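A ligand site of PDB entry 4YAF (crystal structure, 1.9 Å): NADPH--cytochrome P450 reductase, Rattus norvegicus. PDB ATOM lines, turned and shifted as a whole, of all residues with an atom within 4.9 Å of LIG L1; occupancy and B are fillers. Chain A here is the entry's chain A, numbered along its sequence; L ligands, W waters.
The backbone NH (N) of Tyr 399 is in hydrogen-bond range of an oxygen (O9) of LIG L1 (3.4 Å). An oxygen (O9) of LIG L1 sits at hydrogen-bond distance from the backbone carbonyl oxygen (O) of Tyr 399. O13 of LIG L1 is in hydrogen-bond range of N of Thr 435 (2.9 Å). The side-chain hydroxyl (OG1) of Thr 435 sits at hydrogen-bond distance from an oxygen (O13) of LIG L1 (2.7 Å). N of Ala 434 lies within hydrogen-bond range of O14 of LIG L1 (2.7 Å). An oxygen (O11) of LIG L1 sits at hydrogen-bond distance from the side-chain hydroxyl (OH) of Tyr 400. An oxygen (O14) of LIG L1 lies within salt-bridge range of the guanidinium group (NE) of Arg 398 (2.8 Å). O of Cys 416 lies within hydrogen-bond range of N7 of LIG L1, at 2.9 Å. O8 of LIG L1 sits at hydrogen-bond distance from N of Ser 401 (2.9 Å). OG of Ser 401 sits at hydrogen-bond distance from N8 of LIG L1, at 3.4 Å. The backbone NH (N) of Val 433 sits at hydrogen-bond distance from an oxygen (O1) of LIG L1 (3.0 Å). An oxygen (O6) of LIG L1 sits at hydrogen-bond distance from the guanidinium group (NH2) of Arg 368 (3.1 Å). The backbone NH (N) of Val 418 sits at hydrogen-bond distance from an oxygen (O7) of LIG L1 (3.3 Å).
N of Val 420 is in hydrogen-bond range of OG1 of Thr 435, 3.0 Å away. The side-chain hydroxyl (OG) of Ser 401 lies within hydrogen-bond range of the side-chain carboxylate (OD2) of Asp 619, 2.6 Å away. The side-chain hydroxyl (OH) of Tyr 422 is in hydrogen-bond range of the guanidinium group (NE) of Arg 368, at 3.2 Å. OD1 of Asn 323 sits at hydrogen-bond distance from NH1 of Arg 368 (3.1 Å). O of Val 420 lies within hydrogen-bond range of N of Gly 432, at 2.8 Å. OG of Ser 436 is in hydrogen-bond range of O of Gly 432, 2.7 Å away. The side-chain carboxylate (OD1) of Asp 619 is in hydrogen-bond range of a ring nitrogen (NE2) of His 263 (2.9 Å).
His 263 touches LIG L1. Ala 417 touches LIG L1 (CA to O7, 3.1 Å). Val 420 touches LIG L1 (CG1 to C6, 3.8 Å). Tyr 422 touches LIG L1. Gly 432 touches LIG L1. Ala 482 touches LIG L1 (CB to O8, 3.9 Å). CE2 of Trp 621 touches C22 of LIG L1, at 3.3 Å. Hydrophobic or aromatic side chains that line LIG L1: His 263, Tyr 400, Ala 417, Val 420, Tyr 422, Val 433, Ala 434, Ala 482 and Trp 621. Of the 23 residues printed, 17 come within 4 Å of LIG L1. Along chain A the residues within 4 Å of LIG L1 span positions 263 to 621. The nearest printed residue that does not touch LIG L1 is Thr 479 (4.05 Å).
Water W3 bridges an oxygen (O11) of LIG L1 (2.7 Å) and the backbone carbonyl oxygen (O) of Val 418 (2.8 Å). Water W15 lies within hydrogen-bond range of OH of Tyr 422 (2.7 Å), O4 of LIG L1 (2.8 Å) and NH1 of Arg 368 (2.9 Å). Water W11 lies within hydrogen-bond range of OG1 of Thr 322 (2.6 Å), OD1 of Asn 323 (2.8 Å) and O1 of LIG L1 (2.8 Å). Water W10 lies within hydrogen-bond range of O of Ser 401 (2.7 Å), O8 of LIG L1 (2.8 Å) and N of Cys 416 (2.9 Å). Water W5 lies within hydrogen-bond range of the side-chain hydroxyl of Thr 479, an oxygen (O7) of LIG L1 and the indole nitrogen of Trp 621. Water W8 bridges the backbone carbonyl oxygen (O) of Lys 431 (2.7 Å) and an oxygen (O1) of LIG L1 (3.1 Å).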
ATOM      1  N   HIS A 263      14.060 -20.982 -14.249  1.00  0.00           N
ATOM      2  CA  HIS A 263      13.893 -19.700 -13.570  1.00  0.00           C
ATOM      3  C   HIS A 263      13.637 -19.914 -12.085  1.00  0.00           C
ATOM      4  O   HIS A 263      13.043 -20.914 -11.677  1.00  0.00           O
ATOM      5  CB  HIS A 263      12.714 -18.923 -14.155  1.00  0.00           C
ATOM      6  CG  HIS A 263      12.933 -18.484 -15.571  1.00  0.00           C
ATOM      7  ND1 HIS A 263      12.298 -19.087 -16.638  1.00  0.00           N
ATOM      8  CD2 HIS A 263      13.717 -17.519 -16.091  1.00  0.00           C
ATOM      9  CE1 HIS A 263      12.698 -18.504 -17.756  1.00  0.00           C
ATOM     10  NE2 HIS A 263      13.558 -17.551 -17.456  1.00  0.00           N
ATOM     11  N   THR A 322       3.288  -0.501  -5.250  1.00  0.00           N
ATOM     12  CA  THR A 322       4.212   0.278  -6.056  1.00  0.00           C
ATOM     13  C   THR A 322       3.837   0.490  -7.511  1.00  0.00           C
ATOM     14  O   THR A 322       4.297   1.453  -8.120  1.00  0.00           O
ATOM     15  CB  THR A 322       5.609  -0.359  -6.016  1.00  0.00           C
ATOM     16  OG1 THR A 322       5.473  -1.756  -6.278  1.00  0.00           O
ATOM     17  CG2 THR A 322       6.233  -0.178  -4.625  1.00  0.00           C
ATOM     18  N   ASN A 323       3.043  -0.395  -8.087  1.00  0.00           N
ATOM     19  CA  ASN A 323       2.656  -0.202  -9.471  1.00  0.00           C
ATOM     20  C   ASN A 323       1.483   0.768  -9.571  1.00  0.00           C
ATOM     21  O   ASN A 323       0.662   0.840  -8.668  1.00  0.00           O
ATOM     22  CB  ASN A 323       2.355  -1.541 -10.128  1.00  0.00           C
ATOM     23  CG  ASN A 323       3.603  -2.381 -10.323  1.00  0.00           C
ATOM     24  OD1 ASN A 323       4.619  -1.888 -10.830  1.00  0.00           O
ATOM     25  ND2 ASN A 323       3.556  -3.641  -9.898  1.00  0.00           N
ATOM     26  N   ARG A 368       4.275   7.153 -13.337  1.00  0.00           N
ATOM     27  CA  ARG A 368       4.487   6.027 -12.431  1.00  0.00           C
ATOM     28  C   ARG A 368       4.135   6.350 -10.984  1.00  0.00           C
ATOM     29  O   ARG A 368       4.908   6.042 -10.065  1.00  0.00           O
ATOM     30  CB  ARG A 368       5.948   5.568 -12.517  1.00  0.00           C
ATOM     31  CG  ARG A 368       6.324   4.968 -13.859  1.00  0.00           C
ATOM     32  CD  ARG A 368       5.680   3.598 -14.060  1.00  0.00           C
ATOM     33  NE  ARG A 368       6.019   2.684 -12.969  1.00  0.00           N
ATOM     34  CZ  ARG A 368       5.644   1.409 -12.918  1.00  0.00           C
ATOM     35  NH1 ARG A 368       5.989   0.654 -11.874  1.00  0.00           N
ATOM     36  NH2 ARG A 368       4.934   0.879 -13.907  1.00  0.00           N
ATOM     37  N   ARG A 398       8.769 -12.468  -8.311  1.00  0.00           N
ATOM     38  CA  ARG A 398       9.585 -12.003  -9.429  1.00  0.00           C
ATOM     39  C   ARG A 398      10.476 -13.154  -9.894  1.00  0.00           C
ATOM     40  O   ARG A 398      11.029 -13.892  -9.067  1.00  0.00           O
ATOM     41  CB  ARG A 398      10.472 -10.821  -9.026  1.00  0.00           C
ATOM     42  CG  ARG A 398       9.836  -9.441  -9.241  1.00  0.00           C
ATOM     43  CD  ARG A 398       8.664  -9.164  -8.296  1.00  0.00           C
ATOM     44  NE  ARG A 398       8.306  -7.748  -8.321  1.00  0.00           N
ATOM     45  CZ  ARG A 398       7.138  -7.251  -7.927  1.00  0.00           C
ATOM     46  NH1 ARG A 398       6.917  -5.945  -7.985  1.00  0.00           N
ATOM     47  NH2 ARG A 398       6.175  -8.059  -7.489  1.00  0.00           N
ATOM     48  N   TYR A 399      10.624 -13.301 -11.212  1.00  0.00           N
ATOM     49  CA  TYR A 399      11.452 -14.364 -11.792  1.00  0.00           C
ATOM     50  C   TYR A 399      12.823 -13.908 -12.251  1.00  0.00           C
ATOM     51  O   TYR A 399      12.995 -12.803 -12.745  1.00  0.00           O
ATOM     52  CB  TYR A 399      10.721 -14.996 -12.981  1.00  0.00           C
ATOM     53  CG  TYR A 399       9.451 -15.712 -12.593  1.00  0.00           C
ATOM     54  CD1 TYR A 399       8.276 -14.998 -12.360  1.00  0.00           C
ATOM     55  CD2 TYR A 399       9.436 -17.089 -12.415  1.00  0.00           C
ATOM     56  CE1 TYR A 399       7.114 -15.660 -11.951  1.00  0.00           C
ATOM     57  CE2 TYR A 399       8.283 -17.754 -12.016  1.00  0.00           C
ATOM     58  CZ  TYR A 399       7.120 -17.035 -11.782  1.00  0.00           C
ATOM     59  OH  TYR A 399       5.991 -17.687 -11.348  1.00  0.00           O
ATOM     60  N   TYR A 400      13.801 -14.802 -12.072  1.00  0.00           N
ATOM     61  CA  TYR A 400      15.173 -14.549 -12.466  1.00  0.00           C
ATOM     62  C   TYR A 400      15.694 -15.789 -13.177  1.00  0.00           C
ATOM     63  O   TYR A 400      15.334 -16.913 -12.820  1.00  0.00           O
ATOM     64  CB  TYR A 400      16.010 -14.230 -11.224  1.00  0.00           C
ATOM     65  CG  TYR A 400      15.558 -12.941 -10.601  1.00  0.00           C
ATOM     66  CD1 TYR A 400      15.973 -11.712 -11.111  1.00  0.00           C
ATOM     67  CD2 TYR A 400      14.604 -12.932  -9.587  1.00  0.00           C
ATOM     68  CE1 TYR A 400      15.463 -10.514 -10.645  1.00  0.00           C
ATOM     69  CE2 TYR A 400      14.069 -11.727  -9.107  1.00  0.00           C
ATOM     70  CZ  TYR A 400      14.498 -10.534  -9.652  1.00  0.00           C
ATOM     71  OH  TYR A 400      13.936  -9.352  -9.236  1.00  0.00           O
ATOM     72  N   SER A 401      16.527 -15.578 -14.193  1.00  0.00           N
ATOM     73  CA  SER A 401      17.100 -16.680 -14.944  1.00  0.00           C
ATOM     74  C   SER A 401      18.246 -17.247 -14.130  1.00  0.00           C
ATOM     75  O   SER A 401      19.252 -16.572 -13.924  1.00  0.00           O
ATOM     76  CB  SER A 401      17.616 -16.201 -16.296  1.00  0.00           C
ATOM     77  OG  SER A 401      16.570 -15.566 -17.034  1.00  0.00           O
ATOM     78  N   CYS A 416      21.517 -13.171 -11.035  1.00  0.00           N
ATOM     79  CA  CYS A 416      22.197 -12.030 -11.597  1.00  0.00           C
ATOM     80  C   CYS A 416      21.154 -10.971 -11.924  1.00  0.00           C
ATOM     81  O   CYS A 416      20.436 -11.191 -12.804  1.00  0.00           O
ATOM     82  CB  CYS A 416      22.891 -12.429 -12.911  1.00  0.00           C
ATOM     83  SG  CYS A 416      23.583 -11.070 -13.883  1.00  0.00           S
ATOM     84  N   ALA A 417      21.078  -9.869 -11.202  1.00  0.00           N
ATOM     85  CA  ALA A 417      20.067  -8.882 -11.529  1.00  0.00           C
ATOM     86  C   ALA A 417      20.571  -7.467 -11.375  1.00  0.00           C
ATOM     87  O   ALA A 417      21.552  -7.202 -10.680  1.00  0.00           O
ATOM     88  CB  ALA A 417      18.864  -9.088 -10.623  1.00  0.00           C
ATOM     89  N   VAL A 418      19.893  -6.545 -12.055  1.00  0.00           N
ATOM     90  CA  VAL A 418      20.224  -5.145 -11.950  1.00  0.00           C
ATOM     91  C   VAL A 418      19.188  -4.574 -10.986  1.00  0.00           C
ATOM     92  O   VAL A 418      18.006  -4.890 -11.070  1.00  0.00           O
ATOM     93  CB  VAL A 418      20.165  -4.431 -13.336  1.00  0.00           C
ATOM     94  CG1 VAL A 418      18.783  -4.589 -13.976  1.00  0.00           C
ATOM     95  CG2 VAL A 418      20.505  -2.959 -13.157  1.00  0.00           C
ATOM     96  N   VAL A 420      16.675  -2.048  -9.566  1.00  0.00           N
ATOM     97  CA  VAL A 420      15.852  -1.019 -10.190  1.00  0.00           C
ATOM     98  C   VAL A 420      15.683   0.193  -9.274  1.00  0.00           C
ATOM     99  O   VAL A 420      15.239   0.076  -8.140  1.00  0.00           O
ATOM    100  CB  VAL A 420      14.456  -1.582 -10.561  1.00  0.00           C
ATOM    101  CG1 VAL A 420      13.601  -0.500 -11.218  1.00  0.00           C
ATOM    102  CG2 VAL A 420      14.618  -2.767 -11.510  1.00  0.00           C
ATOM    103  N   TYR A 422      14.902   4.439 -10.239  1.00  0.00           N
ATOM    104  CA  TYR A 422      14.852   5.463 -11.264  1.00  0.00           C
ATOM    105  C   TYR A 422      14.041   6.676 -10.881  1.00  0.00           C
ATOM    106  O   TYR A 422      13.231   6.627  -9.945  1.00  0.00           O
ATOM    107  CB  TYR A 422      14.277   4.869 -12.549  1.00  0.00           C
ATOM    108  CG  TYR A 422      12.855   4.365 -12.386  1.00  0.00           C
ATOM    109  CD1 TYR A 422      12.598   3.092 -11.863  1.00  0.00           C
ATOM    110  CD2 TYR A 422      11.770   5.179 -12.711  1.00  0.00           C
ATOM    111  CE1 TYR A 422      11.296   2.647 -11.662  1.00  0.00           C
ATOM    112  CE2 TYR A 422      10.458   4.743 -12.512  1.00  0.00           C
ATOM    113  CZ  TYR A 422      10.227   3.479 -11.987  1.00  0.00           C
ATOM    114  OH  TYR A 422       8.938   3.057 -11.752  1.00  0.00           O
ATOM    115  N   LYS A 431      11.650   2.655  -6.440  1.00  0.00           N
ATOM    116  CA  LYS A 431      12.562   1.550  -6.185  1.00  0.00           C
ATOM    117  C   LYS A 431      11.903   0.230  -6.574  1.00  0.00           C
ATOM    118  O   LYS A 431      10.725   0.021  -6.302  1.00  0.00           O
ATOM    119  CB  LYS A 431      12.929   1.487  -4.701  1.00  0.00           C
ATOM    120  CG  LYS A 431      13.525   2.766  -4.126  1.00  0.00           C
ATOM    121  CD  LYS A 431      14.969   2.965  -4.548  1.00  0.00           C
ATOM    122  CE  LYS A 431      15.870   1.888  -3.958  1.00  0.00           C
ATOM    123  NZ  LYS A 431      15.777   1.853  -2.468  1.00  0.00           N
ATOM    124  N   GLY A 432      12.666  -0.659  -7.210  1.00  0.00           N
ATOM    125  CA  GLY A 432      12.117  -1.951  -7.598  1.00  0.00           C
ATOM    126  C   GLY A 432      11.924  -2.764  -6.335  1.00  0.00           C
ATOM    127  O   GLY A 432      12.818  -2.867  -5.511  1.00  0.00           O
ATOM    128  N   VAL A 433      10.742  -3.354  -6.182  1.00  0.00           N
ATOM    129  CA  VAL A 433      10.424  -4.142  -4.985  1.00  0.00           C
ATOM    130  C   VAL A 433      11.368  -5.313  -4.742  1.00  0.00           C
ATOM    131  O   VAL A 433      12.041  -5.373  -3.710  1.00  0.00           O
ATOM    132  CB  VAL A 433       8.982  -4.703  -5.064  1.00  0.00           C
ATOM    133  CG1 VAL A 433       8.681  -5.547  -3.818  1.00  0.00           C
ATOM    134  CG2 VAL A 433       7.965  -3.556  -5.182  1.00  0.00           C
ATOM    135  N   ALA A 434      11.423  -6.257  -5.677  1.00  0.00           N
ATOM    136  CA  ALA A 434      12.255  -7.442  -5.507  1.00  0.00           C
ATOM    137  C   ALA A 434      13.746  -7.163  -5.472  1.00  0.00           C
ATOM    138  O   ALA A 434      14.468  -7.723  -4.633  1.00  0.00           O
ATOM    139  CB  ALA A 434      11.940  -8.466  -6.594  1.00  0.00           C
ATOM    140  N   THR A 435      14.226  -6.304  -6.359  1.00  0.00           N
ATOM    141  CA  THR A 435      15.652  -6.026  -6.388  1.00  0.00           C
ATOM    142  C   THR A 435      16.141  -5.194  -5.204  1.00  0.00           C
ATOM    143  O   THR A 435      17.266  -5.388  -4.756  1.00  0.00           O
ATOM    144  CB  THR A 435      16.084  -5.391  -7.731  1.00  0.00           C
ATOM    145  OG1 THR A 435      15.334  -4.194  -7.977  1.00  0.00           O
ATOM    146  CG2 THR A 435      15.849  -6.379  -8.874  1.00  0.00           C
ATOM    147  N   SER A 436      15.331  -4.279  -4.692  1.00  0.00           N
ATOM    148  CA  SER A 436      15.791  -3.488  -3.541  1.00  0.00           C
ATOM    149  C   SER A 436      15.884  -4.422  -2.342  1.00  0.00           C
ATOM    150  O   SER A 436      16.830  -4.350  -1.539  1.00  0.00           O
ATOM    151  CB  SER A 436      14.801  -2.353  -3.223  1.00  0.00           C
ATOM    152  OG  SER A 436      14.703  -1.441  -4.297  1.00  0.00           O
ATOM    153  N   THR A 479      22.214  -8.051 -18.447  1.00  0.00           N
ATOM    154  CA  THR A 479      21.776  -9.120 -17.543  1.00  0.00           C
ATOM    155  C   THR A 479      21.357 -10.361 -18.329  1.00  0.00           C
ATOM    156  O   THR A 479      21.027 -11.389 -17.753  1.00  0.00           O
ATOM    157  CB  THR A 479      20.598  -8.671 -16.631  1.00  0.00           C
ATOM    158  OG1 THR A 479      19.529  -8.154 -17.432  1.00  0.00           O
ATOM    159  CG2 THR A 479      21.066  -7.622 -15.637  1.00  0.00           C
ATOM    160  N   ALA A 482      22.914 -13.904 -17.696  1.00  0.00           N
ATOM    161  CA  ALA A 482      22.459 -14.777 -16.614  1.00  0.00           C
ATOM    162  C   ALA A 482      22.429 -16.292 -16.828  1.00  0.00           C
ATOM    163  O   ALA A 482      23.202 -17.029 -16.203  1.00  0.00           O
ATOM    164  CB  ALA A 482      21.093 -14.310 -16.106  1.00  0.00           C
ATOM    165  N   ASP A 619      14.831 -16.149 -23.955  1.00  0.00           N
ATOM    166  CA  ASP A 619      14.641 -15.919 -22.535  1.00  0.00           C
ATOM    167  C   ASP A 619      14.775 -14.406 -22.421  1.00  0.00           C
ATOM    168  O   ASP A 619      15.767 -13.887 -21.918  1.00  0.00           O
ATOM    169  CB  ASP A 619      15.720 -16.616 -21.705  1.00  0.00           C
ATOM    170  CG  ASP A 619      15.520 -16.434 -20.204  1.00  0.00           C
ATOM    171  OD1 ASP A 619      14.400 -16.081 -19.777  1.00  0.00           O
ATOM    172  OD2 ASP A 619      16.484 -16.644 -19.442  1.00  0.00           O
ATOM    173  N   TRP A 621      12.833 -10.518 -21.536  1.00  0.00           N
ATOM    174  CA  TRP A 621      11.839  -9.923 -20.676  1.00  0.00           C
ATOM    175  C   TRP A 621      11.886  -8.400 -20.706  1.00  0.00           C
ATOM    176  O   TRP A 621      12.775  -7.806 -21.330  1.00  0.00           O
ATOM    177  CB  TRP A 621      12.053 -10.402 -19.239  1.00  0.00           C
ATOM    178  CG  TRP A 621      13.371  -9.990 -18.647  1.00  0.00           C
ATOM    179  CD1 TRP A 621      13.674  -8.795 -18.054  1.00  0.00           C
ATOM    180  CD2 TRP A 621      14.581 -10.751 -18.638  1.00  0.00           C
ATOM    181  NE1 TRP A 621      14.991  -8.759 -17.674  1.00  0.00           N
ATOM    182  CE2 TRP A 621      15.578  -9.961 -18.015  1.00  0.00           C
ATOM    183  CE3 TRP A 621      14.931 -12.032 -19.085  1.00  0.00           C
ATOM    184  CZ2 TRP A 621      16.889 -10.392 -17.837  1.00  0.00           C
ATOM    185  CZ3 TRP A 621      16.247 -12.479 -18.899  1.00  0.00           C
ATOM    186  CH2 TRP A 621      17.209 -11.652 -18.278  1.00  0.00           C
HETATM  187  P1  LIG L   1       9.371  -3.684  -9.830  1.00  0.00           P
HETATM  188  O1  LIG L   1       8.994  -3.047  -8.556  1.00  0.00           O
HETATM  189  O2  LIG L   1       8.616  -4.869 -10.291  1.00  0.00           O
HETATM  190  O3  LIG L   1       9.341  -2.569 -10.986  1.00  0.00           O
HETATM  191  C1  LIG L   1       9.450  -2.938 -12.363  1.00  0.00           C
HETATM  192  C2  LIG L   1       8.825  -1.841 -13.216  1.00  0.00           C
HETATM  193  O4  LIG L   1       9.459  -0.575 -12.986  1.00  0.00           O
HETATM  194  C3  LIG L   1       9.106  -2.066 -14.693  1.00  0.00           C
HETATM  195  O5  LIG L   1       8.222  -3.091 -15.184  1.00  0.00           O
HETATM  196  C4  LIG L   1       8.641  -0.721 -15.210  1.00  0.00           C
HETATM  197  O6  LIG L   1       7.210  -0.678 -15.241  1.00  0.00           O
HETATM  198  C5  LIG L   1       9.158   0.240 -14.131  1.00  0.00           C
HETATM  199  N1  LIG L   1      10.421   0.890 -14.535  1.00  0.00           N
HETATM  200  C6  LIG L   1      11.778   0.335 -14.409  1.00  0.00           C
HETATM  201  N2  LIG L   1      12.585   1.449 -14.922  1.00  0.00           N
HETATM  202  C7  LIG L   1      11.774   2.446 -15.260  1.00  0.00           C
HETATM  203  C8  LIG L   1      12.073   3.640 -15.765  1.00  0.00           C
HETATM  204  N3  LIG L   1      13.371   3.947 -15.827  1.00  0.00           N
HETATM  205  N4  LIG L   1      11.139   4.521 -16.130  1.00  0.00           N
HETATM  206  C9  LIG L   1       9.792   4.190 -15.970  1.00  0.00           C
HETATM  207  N5  LIG L   1       9.503   2.922 -15.455  1.00  0.00           N
HETATM  208  C10 LIG L   1      10.498   2.085 -15.107  1.00  0.00           C
HETATM  209  N6  LIG L   1      15.780  -9.479 -14.241  1.00  0.00           N
HETATM  210  C11 LIG L   1      17.140  -9.558 -13.908  1.00  0.00           C
HETATM  211  O7  LIG L   1      17.738  -8.553 -13.534  1.00  0.00           O
HETATM  212  N7  LIG L   1      17.821 -10.774 -14.069  1.00  0.00           N
HETATM  213  C12 LIG L   1      17.157 -11.890 -14.594  1.00  0.00           C
HETATM  214  O8  LIG L   1      17.762 -12.962 -14.698  1.00  0.00           O
HETATM  215  C13 LIG L   1      15.816 -11.801 -14.933  1.00  0.00           C
HETATM  216  N8  LIG L   1      15.211 -12.809 -15.570  1.00  0.00           N
HETATM  217  C14 LIG L   1      13.906 -12.719 -15.888  1.00  0.00           C
HETATM  218  C15 LIG L   1      13.271 -13.798 -16.502  1.00  0.00           C
HETATM  219  C16 LIG L   1      11.920 -13.731 -16.786  1.00  0.00           C
HETATM  220  C17 LIG L   1      11.258 -14.857 -17.268  1.00  0.00           C
HETATM  221  C18 LIG L   1      11.194 -12.578 -16.475  1.00  0.00           C
HETATM  222  C19 LIG L   1       9.834 -12.508 -16.749  1.00  0.00           C
HETATM  223  C20 LIG L   1      11.833 -11.513 -15.853  1.00  0.00           C
HETATM  224  C21 LIG L   1      13.183 -11.578 -15.552  1.00  0.00           C
HETATM  225  N9  LIG L   1      13.796 -10.571 -14.908  1.00  0.00           N
HETATM  226  C22 LIG L   1      15.127 -10.604 -14.764  1.00  0.00           C
HETATM  227  C23 LIG L   1      13.071  -9.350 -14.500  1.00  0.00           C
HETATM  228  C24 LIG L   1      12.616  -9.505 -13.041  1.00  0.00           C
HETATM  229  O9  LIG L   1      11.647 -10.542 -12.955  1.00  0.00           O
HETATM  230  C25 LIG L   1      12.024  -8.214 -12.472  1.00  0.00           C
HETATM  231  O10 LIG L   1      11.021  -7.703 -13.348  1.00  0.00           O
HETATM  232  C26 LIG L   1      13.103  -7.147 -12.253  1.00  0.00           C
HETATM  233  O11 LIG L   1      14.154  -7.658 -11.430  1.00  0.00           O
HETATM  234  C27 LIG L   1      12.468  -5.923 -11.569  1.00  0.00           C
HETATM  235  O12 LIG L   1      11.742  -6.351 -10.412  1.00  0.00           O
HETATM  236  P2  LIG L   1      11.535  -5.386  -9.138  1.00  0.00           P
HETATM  237  O13 LIG L   1      12.863  -5.065  -8.569  1.00  0.00           O
HETATM  238  O14 LIG L   1      10.527  -6.002  -8.247  1.00  0.00           O
HETATM  239  O15 LIG L   1      10.947  -4.037  -9.789  1.00  0.00           O
HETATM  240  N1  LG2 L   2       2.274 -12.050 -24.861  1.00  0.00           N
HETATM  241  C1  LG2 L   2       1.972 -12.532 -26.076  1.00  0.00           C
HETATM  242  O1  LG2 L   2       1.102 -12.000 -26.767  1.00  0.00           O
HETATM  243  N2  LG2 L   2       2.679 -13.636 -26.510  1.00  0.00           N
HETATM  244  C2  LG2 L   2       3.697 -14.312 -25.806  1.00  0.00           C
HETATM  245  O2  LG2 L   2       4.185 -15.279 -26.399  1.00  0.00           O
HETATM  246  C3  LG2 L   2       4.033 -13.808 -24.521  1.00  0.00           C
HETATM  247  N3  LG2 L   2       5.051 -14.468 -23.800  1.00  0.00           N
HETATM  248  C4  LG2 L   2       5.329 -13.898 -22.546  1.00  0.00           C
HETATM  249  C5  LG2 L   2       6.371 -14.545 -21.790  1.00  0.00           C
HETATM  250  C6  LG2 L   2       6.751 -14.080 -20.513  1.00  0.00           C
HETATM  251  C7  LG2 L   2       7.901 -14.856 -19.820  1.00  0.00           C
HETATM  252  C8  LG2 L   2       6.069 -12.884 -19.900  1.00  0.00           C
HETATM  253  C9  LG2 L   2       6.356 -12.339 -18.660  1.00  0.00           C
HETATM  254  C10 LG2 L   2       5.059 -12.269 -20.621  1.00  0.00           C
HETATM  255  C11 LG2 L   2       4.654 -12.741 -21.945  1.00  0.00           C
HETATM  256  N4  LG2 L   2       3.595 -12.120 -22.776  1.00  0.00           N
HETATM  257  C12 LG2 L   2       3.268 -12.666 -24.107  1.00  0.00           C
HETATM  258  C13 LG2 L   2       2.858 -10.961 -22.286  1.00  0.00           C
HETATM  259  C14 LG2 L   2       1.642 -11.324 -21.386  1.00  0.00           C
HETATM  260  O3  LG2 L   2       0.704 -12.178 -22.159  1.00  0.00           O
HETATM  261  C15 LG2 L   2       0.943 -10.058 -20.911  1.00  0.00           C
HETATM  262  O4  LG2 L   2       1.921  -9.294 -20.164  1.00  0.00           O
HETATM  263  C16 LG2 L   2      -0.286 -10.448 -20.015  1.00  0.00           C
HETATM  264  O5  LG2 L   2      -0.811  -9.123 -19.682  1.00  0.00           O
HETATM  265  C17 LG2 L   2       0.073 -11.090 -18.686  1.00  0.00           C
HETATM  266  O6  LG2 L   2      -1.139 -11.451 -17.896  1.00  0.00           O
HETATM  267  P1  LG2 L   2      -1.165 -12.078 -16.465  1.00  0.00           P
HETATM  268  O7  LG2 L   2      -0.636 -11.093 -15.487  1.00  0.00           O
HETATM  269  O8  LG2 L   2      -0.461 -13.472 -16.614  1.00  0.00           O
HETATM  270  O9  LG2 L   2      -2.744 -12.231 -16.218  1.00  0.00           O
HETATM  271  O   HOH W   1       9.140   1.154 -18.438  1.00  0.00           O
HETATM  272  O   HOH W   2      15.196   0.634 -14.532  1.00  0.00           O
HETATM  273  O   HOH W   3      16.251  -6.474 -12.585  1.00  0.00           O
HETATM  274  O   HOH W   4       5.902  -5.005 -11.120  1.00  0.00           O
HETATM  275  O   HOH W   5      17.387  -7.096 -16.190  1.00  0.00           O
HETATM  276  O   HOH W   6       5.554  -3.864 -13.593  1.00  0.00           O
HETATM  277  O   HOH W   7       9.091 -11.238 -12.916  1.00  0.00           O
HETATM  278  O   HOH W   8       8.622  -0.056  -8.068  1.00  0.00           O
HETATM  279  O   HOH W   9       8.251  -3.282 -18.276  1.00  0.00           O
HETATM  280  O   HOH W  10      19.435 -14.157 -12.727  1.00  0.00           O
HETATM  281  O   HOH W  11       6.271  -2.324  -8.636  1.00  0.00           O
HETATM  282  O   HOH W  12       9.407  -8.852 -15.451  1.00  0.00           O
HETATM  283  O   HOH W  13       8.770  -7.044 -11.958  1.00  0.00           O
HETATM  284  O   HOH W  14      11.016  -5.544 -15.098  1.00  0.00           O
HETATM  285  O   HOH W  15       8.564   0.592 -10.626  1.00  0.00           O
